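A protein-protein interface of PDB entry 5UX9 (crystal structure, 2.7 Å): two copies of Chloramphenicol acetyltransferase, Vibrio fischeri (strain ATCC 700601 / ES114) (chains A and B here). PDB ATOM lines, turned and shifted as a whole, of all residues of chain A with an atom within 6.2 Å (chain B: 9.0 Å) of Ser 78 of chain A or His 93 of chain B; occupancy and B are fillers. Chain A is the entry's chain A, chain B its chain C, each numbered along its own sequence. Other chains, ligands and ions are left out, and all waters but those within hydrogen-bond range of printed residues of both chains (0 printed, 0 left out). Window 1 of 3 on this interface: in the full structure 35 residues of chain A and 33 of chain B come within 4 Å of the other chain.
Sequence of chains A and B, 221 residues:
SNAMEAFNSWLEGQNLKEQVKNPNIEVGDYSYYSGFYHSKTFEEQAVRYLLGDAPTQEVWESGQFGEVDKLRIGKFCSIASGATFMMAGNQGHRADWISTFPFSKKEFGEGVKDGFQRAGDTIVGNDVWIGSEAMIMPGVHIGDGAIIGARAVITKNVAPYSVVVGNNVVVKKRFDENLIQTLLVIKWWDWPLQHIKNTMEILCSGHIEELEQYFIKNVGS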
ATOM      1  N   SER A  31      16.776 -20.175   6.284  1.00  0.00           N
ATOM      2  CA  SER A  31      17.734 -19.298   5.623  1.00  0.00           C
ATOM      3  C   SER A  31      18.415 -18.400   6.651  1.00  0.00           C
ATOM      4  O   SER A  31      17.750 -17.771   7.481  1.00  0.00           O
ATOM      5  CB  SER A  31      17.038 -18.456   4.556  1.00  0.00           C
ATOM      6  OG  SER A  31      16.332 -19.276   3.642  1.00  0.00           O
ATOM      7  N   TYR A  32      19.743 -18.339   6.592  1.00  0.00           N
ATOM      8  CA  TYR A  32      20.535 -17.646   7.596  1.00  0.00           C
ATOM      9  C   TYR A  32      21.423 -16.587   6.957  1.00  0.00           C
ATOM     10  O   TYR A  32      21.685 -16.600   5.751  1.00  0.00           O
ATOM     11  CB  TYR A  32      21.407 -18.628   8.393  1.00  0.00           C
ATOM     12  CG  TYR A  32      22.560 -19.215   7.602  1.00  0.00           C
ATOM     13  CD1 TYR A  32      23.821 -18.627   7.627  1.00  0.00           C
ATOM     14  CD2 TYR A  32      22.390 -20.360   6.838  1.00  0.00           C
ATOM     15  CE1 TYR A  32      24.874 -19.161   6.907  1.00  0.00           C
ATOM     16  CE2 TYR A  32      23.437 -20.902   6.117  1.00  0.00           C
ATOM     17  CZ  TYR A  32      24.676 -20.300   6.155  1.00  0.00           C
ATOM     18  OH  TYR A  32      25.719 -20.839   5.437  1.00  0.00           O
ATOM     19  N   PHE A  76      16.135 -22.258   2.929  1.00  0.00           N
ATOM     20  CA  PHE A  76      17.437 -22.931   2.920  1.00  0.00           C
ATOM     21  C   PHE A  76      18.480 -22.137   2.136  1.00  0.00           C
ATOM     22  O   PHE A  76      19.249 -22.694   1.348  1.00  0.00           O
ATOM     23  CB  PHE A  76      17.315 -24.354   2.369  1.00  0.00           C
ATOM     24  CG  PHE A  76      16.442 -25.254   3.195  1.00  0.00           C
ATOM     25  CD1 PHE A  76      16.961 -25.935   4.285  1.00  0.00           C
ATOM     26  CD2 PHE A  76      15.105 -25.422   2.880  1.00  0.00           C
ATOM     27  CE1 PHE A  76      16.160 -26.767   5.046  1.00  0.00           C
ATOM     28  CE2 PHE A  76      14.299 -26.253   3.636  1.00  0.00           C
ATOM     29  CZ  PHE A  76      14.827 -26.926   4.721  1.00  0.00           C
ATOM     30  N   CYS A  77      18.512 -20.828   2.350  1.00  0.00           N
ATOM     31  CA  CYS A  77      19.455 -19.958   1.666  1.00  0.00           C
ATOM     32  C   CYS A  77      20.641 -19.653   2.571  1.00  0.00           C
ATOM     33  O   CYS A  77      20.486 -19.493   3.784  1.00  0.00           O
ATOM     34  CB  CYS A  77      18.776 -18.660   1.226  1.00  0.00           C
ATOM     35  SG  CYS A  77      17.638 -18.872  -0.160  1.00  0.00           S
ATOM     36  N   SER A  78      21.826 -19.582   1.972  1.00  0.00           N
ATOM     37  CA  SER A  78      23.063 -19.275   2.684  1.00  0.00           C
ATOM     38  C   SER A  78      23.582 -17.936   2.175  1.00  0.00           C
ATOM     39  O   SER A  78      23.980 -17.819   1.010  1.00  0.00           O
ATOM     40  CB  SER A  78      24.100 -20.378   2.486  1.00  0.00           C
ATOM     41  OG  SER A  78      23.521 -21.660   2.650  1.00  0.00           O
ATOM     42  N   ILE A  79      23.577 -16.930   3.044  1.00  0.00           N
ATOM     43  CA  ILE A  79      24.042 -15.587   2.713  1.00  0.00           C
ATOM     44  C   ILE A  79      25.271 -15.291   3.562  1.00  0.00           C
ATOM     45  O   ILE A  79      25.182 -15.217   4.795  1.00  0.00           O
ATOM     46  CB  ILE A  79      22.946 -14.535   2.938  1.00  0.00           C
ATOM     47  CG1 ILE A  79      21.809 -14.732   1.934  1.00  0.00           C
ATOM     48  CG2 ILE A  79      23.519 -13.136   2.819  1.00  0.00           C
ATOM     49  CD1 ILE A  79      20.478 -14.195   2.408  1.00  0.00           C
ATOM     50  N   ALA A  80      26.415 -15.119   2.903  1.00  0.00           N
ATOM     51  CA  ALA A  80      27.674 -14.898   3.593  1.00  0.00           C
ATOM     52  C   ALA A  80      27.834 -13.427   3.977  1.00  0.00           C
ATOM     53  O   ALA A  80      27.027 -12.564   3.616  1.00  0.00           O
ATOM     54  CB  ALA A  80      28.846 -15.352   2.726  1.00  0.00           C
ATOM     55  N   ASP A 127      17.395 -22.577  -1.750  1.00  0.00           N
ATOM     56  CA  ASP A 127      18.686 -23.264  -1.836  1.00  0.00           C
ATOM     57  C   ASP A 127      19.719 -22.409  -2.568  1.00  0.00           C
ATOM     58  O   ASP A 127      20.478 -22.895  -3.410  1.00  0.00           O
ATOM     59  CB  ASP A 127      18.536 -24.638  -2.502  1.00  0.00           C
ATOM     60  CG  ASP A 127      19.746 -25.533  -2.285  1.00  0.00           C
ATOM     61  OD1 ASP A 127      20.256 -25.586  -1.145  1.00  0.00           O
ATOM     62  OD2 ASP A 127      20.183 -26.187  -3.256  1.00  0.00           O
ATOM     63  N   VAL A 128      19.751 -21.120  -2.247  1.00  0.00           N
ATOM     64  CA  VAL A 128      20.652 -20.171  -2.890  1.00  0.00           C
ATOM     65  C   VAL A 128      21.817 -19.884  -1.951  1.00  0.00           C
ATOM     66  O   VAL A 128      21.614 -19.589  -0.766  1.00  0.00           O
ATOM     67  CB  VAL A 128      19.917 -18.875  -3.272  1.00  0.00           C
ATOM     68  CG1 VAL A 128      20.904 -17.832  -3.770  1.00  0.00           C
ATOM     69  CG2 VAL A 128      18.859 -19.162  -4.326  1.00  0.00           C
ATOM     70  N   TRP A 129      23.036 -19.987  -2.476  1.00  0.00           N
ATOM     71  CA  TRP A 129      24.256 -19.649  -1.750  1.00  0.00           C
ATOM     72  C   TRP A 129      24.848 -18.404  -2.398  1.00  0.00           C
ATOM     73  O   TRP A 129      25.274 -18.444  -3.557  1.00  0.00           O
ATOM     74  CB  TRP A 129      25.248 -20.812  -1.765  1.00  0.00           C
ATOM     75  CG  TRP A 129      26.595 -20.475  -1.178  1.00  0.00           C
ATOM     76  CD1 TRP A 129      26.862 -19.551  -0.206  1.00  0.00           C
ATOM     77  CD2 TRP A 129      27.856 -21.055  -1.534  1.00  0.00           C
ATOM     78  NE1 TRP A 129      28.209 -19.524   0.064  1.00  0.00           N
ATOM     79  CE2 TRP A 129      28.841 -20.437  -0.737  1.00  0.00           C
ATOM     80  CE3 TRP A 129      28.248 -22.038  -2.449  1.00  0.00           C
ATOM     81  CZ2 TRP A 129      30.192 -20.769  -0.828  1.00  0.00           C
ATOM     82  CZ3 TRP A 129      29.591 -22.367  -2.536  1.00  0.00           C
ATOM     83  CH2 TRP A 129      30.546 -21.734  -1.731  1.00  0.00           C
ATOM     84  N   ILE A 130      24.860 -17.302  -1.651  1.00  0.00           N
ATOM     85  CA  ILE A 130      25.385 -16.021  -2.110  1.00  0.00           C
ATOM     86  C   ILE A 130      26.695 -15.772  -1.375  1.00  0.00           C
ATOM     87  O   ILE A 130      26.712 -15.670  -0.143  1.00  0.00           O
ATOM     88  CB  ILE A 130      24.380 -14.881  -1.877  1.00  0.00           C
ATOM     89  CG1 ILE A 130      23.016 -15.234  -2.480  1.00  0.00           C
ATOM     90  CG2 ILE A 130      24.904 -13.558  -2.440  1.00  0.00           C
ATOM     91  CD1 ILE A 130      22.026 -14.089  -2.454  1.00  0.00           C
ATOM     92  N   GLY A 131      27.792 -15.697  -2.133  1.00  0.00           N
ATOM     93  CA  GLY A 131      29.111 -15.548  -1.552  1.00  0.00           C
ATOM     94  C   GLY A 131      29.304 -14.233  -0.818  1.00  0.00           C
ATOM     95  O   GLY A 131      28.480 -13.321  -0.869  1.00  0.00           O
ATOM     96  N   TYR B  49      37.827 -16.540   8.566  1.00  0.00           N
ATOM     97  CA  TYR B  49      37.425 -17.944   8.653  1.00  0.00           C
ATOM     98  C   TYR B  49      38.611 -18.868   8.912  1.00  0.00           C
ATOM     99  O   TYR B  49      38.576 -20.052   8.571  1.00  0.00           O
ATOM    100  CB  TYR B  49      36.667 -18.384   7.397  1.00  0.00           C
ATOM    101  CG  TYR B  49      35.600 -17.409   6.957  1.00  0.00           C
ATOM    102  CD1 TYR B  49      34.400 -17.309   7.645  1.00  0.00           C
ATOM    103  CD2 TYR B  49      35.792 -16.591   5.851  1.00  0.00           C
ATOM    104  CE1 TYR B  49      33.421 -16.423   7.249  1.00  0.00           C
ATOM    105  CE2 TYR B  49      34.817 -15.700   5.448  1.00  0.00           C
ATOM    106  CZ  TYR B  49      33.633 -15.618   6.148  1.00  0.00           C
ATOM    107  OH  TYR B  49      32.660 -14.731   5.745  1.00  0.00           O
ATOM    108  N   ALA B  88      39.180 -21.443   5.301  1.00  0.00           N
ATOM    109  CA  ALA B  88      38.152 -22.441   5.596  1.00  0.00           C
ATOM    110  C   ALA B  88      37.619 -23.137   4.346  1.00  0.00           C
ATOM    111  O   ALA B  88      36.581 -23.803   4.407  1.00  0.00           O
ATOM    112  CB  ALA B  88      36.990 -21.832   6.389  1.00  0.00           C
ATOM    113  N   GLY B  89      38.308 -22.999   3.214  1.00  0.00           N
ATOM    114  CA  GLY B  89      37.919 -23.731   2.018  1.00  0.00           C
ATOM    115  C   GLY B  89      36.498 -23.417   1.591  1.00  0.00           C
ATOM    116  O   GLY B  89      36.094 -22.253   1.494  1.00  0.00           O
ATOM    117  N   ASN B  90      35.720 -24.472   1.340  1.00  0.00           N
ATOM    118  CA  ASN B  90      34.336 -24.324   0.907  1.00  0.00           C
ATOM    119  C   ASN B  90      33.371 -24.085   2.060  1.00  0.00           C
ATOM    120  O   ASN B  90      32.186 -23.840   1.806  1.00  0.00           O
ATOM    121  CB  ASN B  90      33.896 -25.560   0.117  1.00  0.00           C
ATOM    122  CG  ASN B  90      33.916 -26.827   0.954  1.00  0.00           C
ATOM    123  OD1 ASN B  90      34.520 -26.870   2.025  1.00  0.00           O
ATOM    124  ND2 ASN B  90      33.253 -27.868   0.463  1.00  0.00           N
ATOM    125  N   GLN B  91      33.842 -24.161   3.307  1.00  0.00           N
ATOM    126  CA  GLN B  91      33.024 -23.890   4.491  1.00  0.00           C
ATOM    127  C   GLN B  91      31.791 -24.787   4.561  1.00  0.00           C
ATOM    128  O   GLN B  91      30.740 -24.379   5.064  1.00  0.00           O
ATOM    129  CB  GLN B  91      32.611 -22.417   4.551  1.00  0.00           C
ATOM    130  CG  GLN B  91      33.780 -21.454   4.559  1.00  0.00           C
ATOM    131  CD  GLN B  91      33.353 -20.023   4.813  1.00  0.00           C
ATOM    132  OE1 GLN B  91      32.450 -19.763   5.608  1.00  0.00           O
ATOM    133  NE2 GLN B  91      34.004 -19.085   4.137  1.00  0.00           N
ATOM    134  N   GLY B  92      31.904 -26.017   4.063  1.00  0.00           N
ATOM    135  CA  GLY B  92      30.810 -26.960   4.097  1.00  0.00           C
ATOM    136  C   GLY B  92      29.850 -26.881   2.930  1.00  0.00           C
ATOM    137  O   GLY B  92      29.043 -27.801   2.751  1.00  0.00           O
ATOM    138  N   HIS B  93      29.901 -25.815   2.136  1.00  0.00           N
ATOM    139  CA  HIS B  93      29.039 -25.699   0.967  1.00  0.00           C
ATOM    140  C   HIS B  93      29.592 -26.553  -0.166  1.00  0.00           C
ATOM    141  O   HIS B  93      30.757 -26.411  -0.549  1.00  0.00           O
ATOM    142  CB  HIS B  93      28.922 -24.239   0.532  1.00  0.00           C
ATOM    143  CG  HIS B  93      28.497 -23.314   1.630  1.00  0.00           C
ATOM    144  ND1 HIS B  93      27.224 -23.318   2.157  1.00  0.00           N
ATOM    145  CD2 HIS B  93      29.179 -22.355   2.302  1.00  0.00           C
ATOM    146  CE1 HIS B  93      27.138 -22.403   3.105  1.00  0.00           C
ATOM    147  NE2 HIS B  93      28.311 -21.804   3.214  1.00  0.00           N
ATOM    148  N   ARG B  94      28.757 -27.442  -0.699  1.00  0.00           N
ATOM    149  CA  ARG B  94      29.156 -28.367  -1.757  1.00  0.00           C
ATOM    150  C   ARG B  94      28.316 -28.091  -2.997  1.00  0.00           C
ATOM    151  O   ARG B  94      27.122 -28.405  -3.027  1.00  0.00           O
ATOM    152  CB  ARG B  94      29.001 -29.817  -1.304  1.00  0.00           C
ATOM    153  CG  ARG B  94      30.015 -30.237  -0.261  1.00  0.00           C
ATOM    154  CD  ARG B  94      31.307 -30.704  -0.907  1.00  0.00           C
ATOM    155  NE  ARG B  94      31.119 -31.931  -1.673  1.00  0.00           N
ATOM    156  CZ  ARG B  94      31.997 -32.926  -1.716  1.00  0.00           C
ATOM    157  NH1 ARG B  94      33.130 -32.843  -1.030  1.00  0.00           N
ATOM    158  NH2 ARG B  94      31.742 -34.007  -2.439  1.00  0.00           N
ATOM    159  N   ALA B  95      28.946 -27.509  -4.020  1.00  0.00           N
ATOM    160  CA  ALA B  95      28.235 -27.231  -5.263  1.00  0.00           C
ATOM    161  C   ALA B  95      27.834 -28.513  -5.981  1.00  0.00           C
ATOM    162  O   ALA B  95      26.835 -28.526  -6.711  1.00  0.00           O
ATOM    163  CB  ALA B  95      29.095 -26.359  -6.175  1.00  0.00           C
ATOM    164  N   ASP B  96      28.589 -29.594  -5.787  1.00  0.00           N
ATOM    165  CA  ASP B  96      28.286 -30.867  -6.427  1.00  0.00           C
ATOM    166  C   ASP B  96      27.217 -31.665  -5.692  1.00  0.00           C
ATOM    167  O   ASP B  96      26.792 -32.708  -6.199  1.00  0.00           O
ATOM    168  CB  ASP B  96      29.558 -31.707  -6.555  1.00  0.00           C
ATOM    169  CG  ASP B  96      30.293 -31.854  -5.236  1.00  0.00           C
ATOM    170  OD1 ASP B  96      30.104 -30.994  -4.349  1.00  0.00           O
ATOM    171  OD2 ASP B  96      31.059 -32.831  -5.086  1.00  0.00           O
ATOM    172  N   TRP B  97      26.783 -31.215  -4.521  1.00  0.00           N
ATOM    173  CA  TRP B  97      25.715 -31.885  -3.796  1.00  0.00           C
ATOM    174  C   TRP B  97      24.363 -31.286  -4.170  1.00  0.00           C
ATOM    175  O   TRP B  97      24.275 -30.199  -4.748  1.00  0.00           O
ATOM    176  CB  TRP B  97      25.937 -31.784  -2.286  1.00  0.00           C
ATOM    177  CG  TRP B  97      26.948 -32.756  -1.768  1.00  0.00           C
ATOM    178  CD1 TRP B  97      27.704 -33.623  -2.504  1.00  0.00           C
ATOM    179  CD2 TRP B  97      27.317 -32.964  -0.400  1.00  0.00           C
ATOM    180  NE1 TRP B  97      28.523 -34.356  -1.678  1.00  0.00           N
ATOM    181  CE2 TRP B  97      28.304 -33.970  -0.381  1.00  0.00           C
ATOM    182  CE3 TRP B  97      26.911 -32.396   0.811  1.00  0.00           C
ATOM    183  CZ2 TRP B  97      28.888 -34.421   0.800  1.00  0.00           C
ATOM    184  CZ3 TRP B  97      27.492 -32.845   1.984  1.00  0.00           C
ATOM    185  CH2 TRP B  97      28.469 -33.847   1.970  1.00  0.00           C
ATOM    186  N   SER B  99      22.083 -30.030  -2.291  1.00  0.00           N
ATOM    187  CA  SER B  99      21.886 -28.776  -1.582  1.00  0.00           C
ATOM    188  C   SER B  99      23.223 -28.255  -1.081  1.00  0.00           C
ATOM    189  O   SER B  99      24.045 -29.020  -0.570  1.00  0.00           O
ATOM    190  CB  SER B  99      20.926 -28.946  -0.406  1.00  0.00           C
ATOM    191  OG  SER B  99      20.928 -27.792   0.413  1.00  0.00           O
ATOM    192  N   THR B 100      23.435 -26.951  -1.231  1.00  0.00           N
ATOM    193  CA  THR B 100      24.622 -26.297  -0.701  1.00  0.00           C
ATOM    194  C   THR B 100      24.432 -25.810   0.727  1.00  0.00           C
ATOM    195  O   THR B 100      25.350 -25.206   1.290  1.00  0.00           O
ATOM    196  CB  THR B 100      25.024 -25.114  -1.588  1.00  0.00           C
ATOM    197  OG1 THR B 100      23.956 -24.159  -1.623  1.00  0.00           O
ATOM    198  CG2 THR B 100      25.328 -25.586  -3.003  1.00  0.00           C
ATOM    199  N   PHE B 101      23.272 -26.051   1.317  1.00  0.00           N
ATOM    200  CA  PHE B 101      23.002 -25.561   2.660  1.00  0.00           C
ATOM    201  C   PHE B 101      23.695 -26.449   3.686  1.00  0.00           C
ATOM    202  O   PHE B 101      23.592 -27.678   3.606  1.00  0.00           O
ATOM    203  CB  PHE B 101      21.502 -25.524   2.928  1.00  0.00           C
ATOM    204  CG  PHE B 101      21.139 -24.892   4.237  1.00  0.00           C
ATOM    205  CD1 PHE B 101      21.014 -25.661   5.382  1.00  0.00           C
ATOM    206  CD2 PHE B 101      20.926 -23.527   4.326  1.00  0.00           C
ATOM    207  CE1 PHE B 101      20.683 -25.081   6.591  1.00  0.00           C
ATOM    208  CE2 PHE B 101      20.594 -22.940   5.530  1.00  0.00           C
ATOM    209  CZ  PHE B 101      20.472 -23.718   6.665  1.00  0.00           C
ATOM    210  N   PRO B 102      24.407 -25.873   4.652  1.00  0.00           N
ATOM    211  CA  PRO B 102      25.069 -26.695   5.673  1.00  0.00           C
ATOM    212  C   PRO B 102      24.121 -27.106   6.788  1.00  0.00           C
ATOM    213  O   PRO B 102      24.025 -26.427   7.815  1.00  0.00           O
ATOM    214  CB  PRO B 102      26.186 -25.779   6.183  1.00  0.00           C
ATOM    215  CG  PRO B 102      25.650 -24.400   5.980  1.00  0.00           C
ATOM    216  CD  PRO B 102      24.726 -24.441   4.792  1.00  0.00           C
ATOM    217  N   PHE B 103      23.416 -28.218   6.588  1.00  0.00           N
ATOM    218  CA  PHE B 103      22.486 -28.709   7.596  1.00  0.00           C
ATOM    219  C   PHE B 103      23.230 -29.057   8.881  1.00  0.00           C
ATOM    220  O   PHE B 103      24.350 -29.574   8.849  1.00  0.00           O
ATOM    221  CB  PHE B 103      21.735 -29.936   7.073  1.00  0.00           C
ATOM    222  CG  PHE B 103      21.037 -29.713   5.759  1.00  0.00           C
ATOM    223  CD1 PHE B 103      19.740 -29.223   5.721  1.00  0.00           C
ATOM    224  CD2 PHE B 103      21.675 -30.000   4.561  1.00  0.00           C
ATOM    225  CE1 PHE B 103      19.096 -29.019   4.513  1.00  0.00           C
ATOM    226  CE2 PHE B 103      21.036 -29.796   3.349  1.00  0.00           C
ATOM    227  CZ  PHE B 103      19.745 -29.305   3.326  1.00  0.00           C
ATOM    228  N   LYS B 113      25.672 -35.473   6.490  1.00  0.00           N
ATOM    229  CA  LYS B 113      27.042 -35.684   6.051  1.00  0.00           C
ATOM    230  C   LYS B 113      27.763 -34.343   5.997  1.00  0.00           C
ATOM    231  O   LYS B 113      27.216 -33.352   5.503  1.00  0.00           O
ATOM    232  CB  LYS B 113      27.079 -36.365   4.682  1.00  0.00           C
ATOM    233  CG  LYS B 113      28.470 -36.721   4.182  1.00  0.00           C
ATOM    234  CD  LYS B 113      28.423 -37.916   3.245  1.00  0.00           C
ATOM    235  CE  LYS B 113      29.682 -37.996   2.395  1.00  0.00           C
ATOM    236  NZ  LYS B 113      30.882 -37.496   3.121  1.00  0.00           N
ATOM    237  N   ASP B 114      28.975 -34.289   6.541  1.00  0.00           N
ATOM    238  CA  ASP B 114      29.738 -33.048   6.581  1.00  0.00           C
ATOM    239  C   ASP B 114      30.331 -32.766   5.206  1.00  0.00           C
ATOM    240  O   ASP B 114      31.054 -33.600   4.650  1.00  0.00           O
ATOM    241  CB  ASP B 114      30.834 -33.138   7.638  1.00  0.00           C
ATOM    242  CG  ASP B 114      31.367 -31.783   8.038  1.00  0.00           C
ATOM    243  OD1 ASP B 114      30.673 -30.771   7.800  1.00  0.00           O
ATOM    244  OD2 ASP B 114      32.480 -31.730   8.597  1.00  0.00           O
ATOM    245  N   GLY B 115      30.031 -31.592   4.662  1.00  0.00           N
ATOM    246  CA  GLY B 115      30.464 -31.241   3.330  1.00  0.00           C
ATOM    247  C   GLY B 115      31.760 -30.476   3.233  1.00  0.00           C
ATOM    248  O   GLY B 115      32.211 -30.189   2.121  1.00  0.00           O
ATOM    249  N   PHE B 116      32.381 -30.132   4.359  1.00  0.00           N
ATOM    250  CA  PHE B 116      33.604 -29.349   4.281  1.00  0.00           C
ATOM    251  C   PHE B 116      34.716 -30.161   3.627  1.00  0.00           C
ATOM    252  O   PHE B 116      34.861 -31.361   3.873  1.00  0.00           O
ATOM    253  CB  PHE B 116      34.036 -28.887   5.673  1.00  0.00           C
ATOM    254  CG  PHE B 116      35.464 -28.418   5.740  1.00  0.00           C
ATOM    255  CD1 PHE B 116      35.786 -27.088   5.519  1.00  0.00           C
ATOM    256  CD2 PHE B 116      36.481 -29.306   6.045  1.00  0.00           C
ATOM    257  CE1 PHE B 116      37.098 -26.657   5.589  1.00  0.00           C
ATOM    258  CE2 PHE B 116      37.794 -28.880   6.117  1.00  0.00           C
ATOM    259  CZ  PHE B 116      38.104 -27.554   5.888  1.00  0.00           C
ATOM    260  N   GLN B 117      35.503 -29.476   2.800  1.00  0.00           N
ATOM    261  CA  GLN B 117      36.681 -30.062   2.180  1.00  0.00           C
ATOM    262  C   GLN B 117      37.771 -29.006   2.098  1.00  0.00           C
ATOM    263  O   GLN B 117      37.508 -27.856   1.734  1.00  0.00           O
ATOM    264  CB  GLN B 117      36.377 -30.619   0.781  1.00  0.00           C
ATOM    265  CG  GLN B 117      35.876 -32.057   0.783  1.00  0.00           C
ATOM    266  CD  GLN B 117      36.885 -33.041   1.359  1.00  0.00           C
ATOM    267  OE1 GLN B 117      38.089 -32.778   1.379  1.00  0.00           O
ATOM    268  NE2 GLN B 117      36.394 -34.179   1.835  1.00  0.00           N
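The side-chain carboxylate (OD1) of Asp 127 of chain A is in hydrogen-bond range of the side-chain hydroxyl (OG) of Ser 99 of chain B (2.8 Å). The backbone NH (N) of Thr 100 of chain B sits at hydrogen-bond distance from the side-chain carboxylate (OD1) of Asp 127 of chain A (3.5 Å).
No position is printed for both chains.
Of the 12 printed residues of chain A, 6 touch a printed residue of chain B. Hydrophobic or aromatic side chains of chain A within 4 Å of the printed part of chain B: Tyr 32, Phe 76 and Trp 129. Of the 21 printed residues of chain B, 6 touch a printed residue of chain A. Hydrophobic or aromatic side chains of chain B that line the printed part of chain A: His 93, Phe 101, Pro 102 and Phe 103. Among the printed residues, 14 pairs touch across the chains.
Tyr 32 of chain A touches Pro 102 of chain B. Phe 76 of chain A touches Phe 101 of chain B (O to CD2, 3.5 Å). Phe 103 of chain B touches Phe 76 of chain A (CE1 to CE1, 3.7 Å). Phe 101 of chain B touches Cys 77 of chain A. Ser 78 of chain A touches His 93 of chain B (CB to CE1, 3.7 Å). OG of Ser 78 of chain A touches CD2 of Phe 101 of chain B, 3.6 Å away. Ser 78 of chain A touches Pro 102 of chain B (OG to CD, 3.7 Å). OD1 of Asp 127 of chain A touches N of Phe 101 of chain B, at 3.9 Å. His 93 of chain B touches Trp 129 of chain A. Trp 129 of chain A touches Thr 100 of chain B.
Ser 78 of chain A touches just these residues of chain B: His 93 (3.7 Å), Phe 101 (3.6 Å) and Pro 102 (3.7 Å). Of the printed residues of chain A, His 93 of chain B touches Tyr 32 (3.1 Å), Ser 78 (3.7 Å) and Trp 129 (3.6 Å). No residue of chain B comes within 4 Å of Ile 79 of chain A. Trp 129 of chain A touches two residues of chain B. Printed residues of chain B within 4 Å of Asp 127 of chain A: Ser 99, Thr 100 and Phe 101. Of the printed residues of chain A, Ser 99 of chain B touches Asp 127 (2.8 Å). Printed residues of chain B within 4 Å of Phe 76 of chain A: Phe 101 (3.5 Å) and Phe 103 (3.7 Å). Ala 80 of chain A touches none of the printed residues of chain B. The nearest residue of chain B that does not touch Ser 78 of chain A is Thr 100 of chain B (4.2 Å). The nearest printed residue of chain A that does not touch His 93 of chain B is Ala 80 of chain A (6.5 Å).
The backbone NH (N) of Tyr 32 of chain A sits at hydrogen-bond distance from the backbone carbonyl oxygen (O) of Cys 77 of chain A, 3.1 Å away. The backbone NH (N) of Ser 78 of chain A is in hydrogen-bond range of the backbone carbonyl oxygen (O) of Val 128 of chain A (2.7 Å). The backbone carbonyl oxygen (O) of Ser 78 of chain A is in hydrogen-bond range of the backbone NH (N) of Ile 130 of chain A (2.9 Å). ND2 of Asn 90 of chain B is in hydrogen-bond range of O of His 93 of chain B, at 3.1 Å. O of Thr 100 of chain B is in hydrogen-bond range of ND1 of His 93 of chain B. N of Phe 101 of chain B sits at hydrogen-bond distance from OG of Ser 99 of chain B (3.1 Å).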
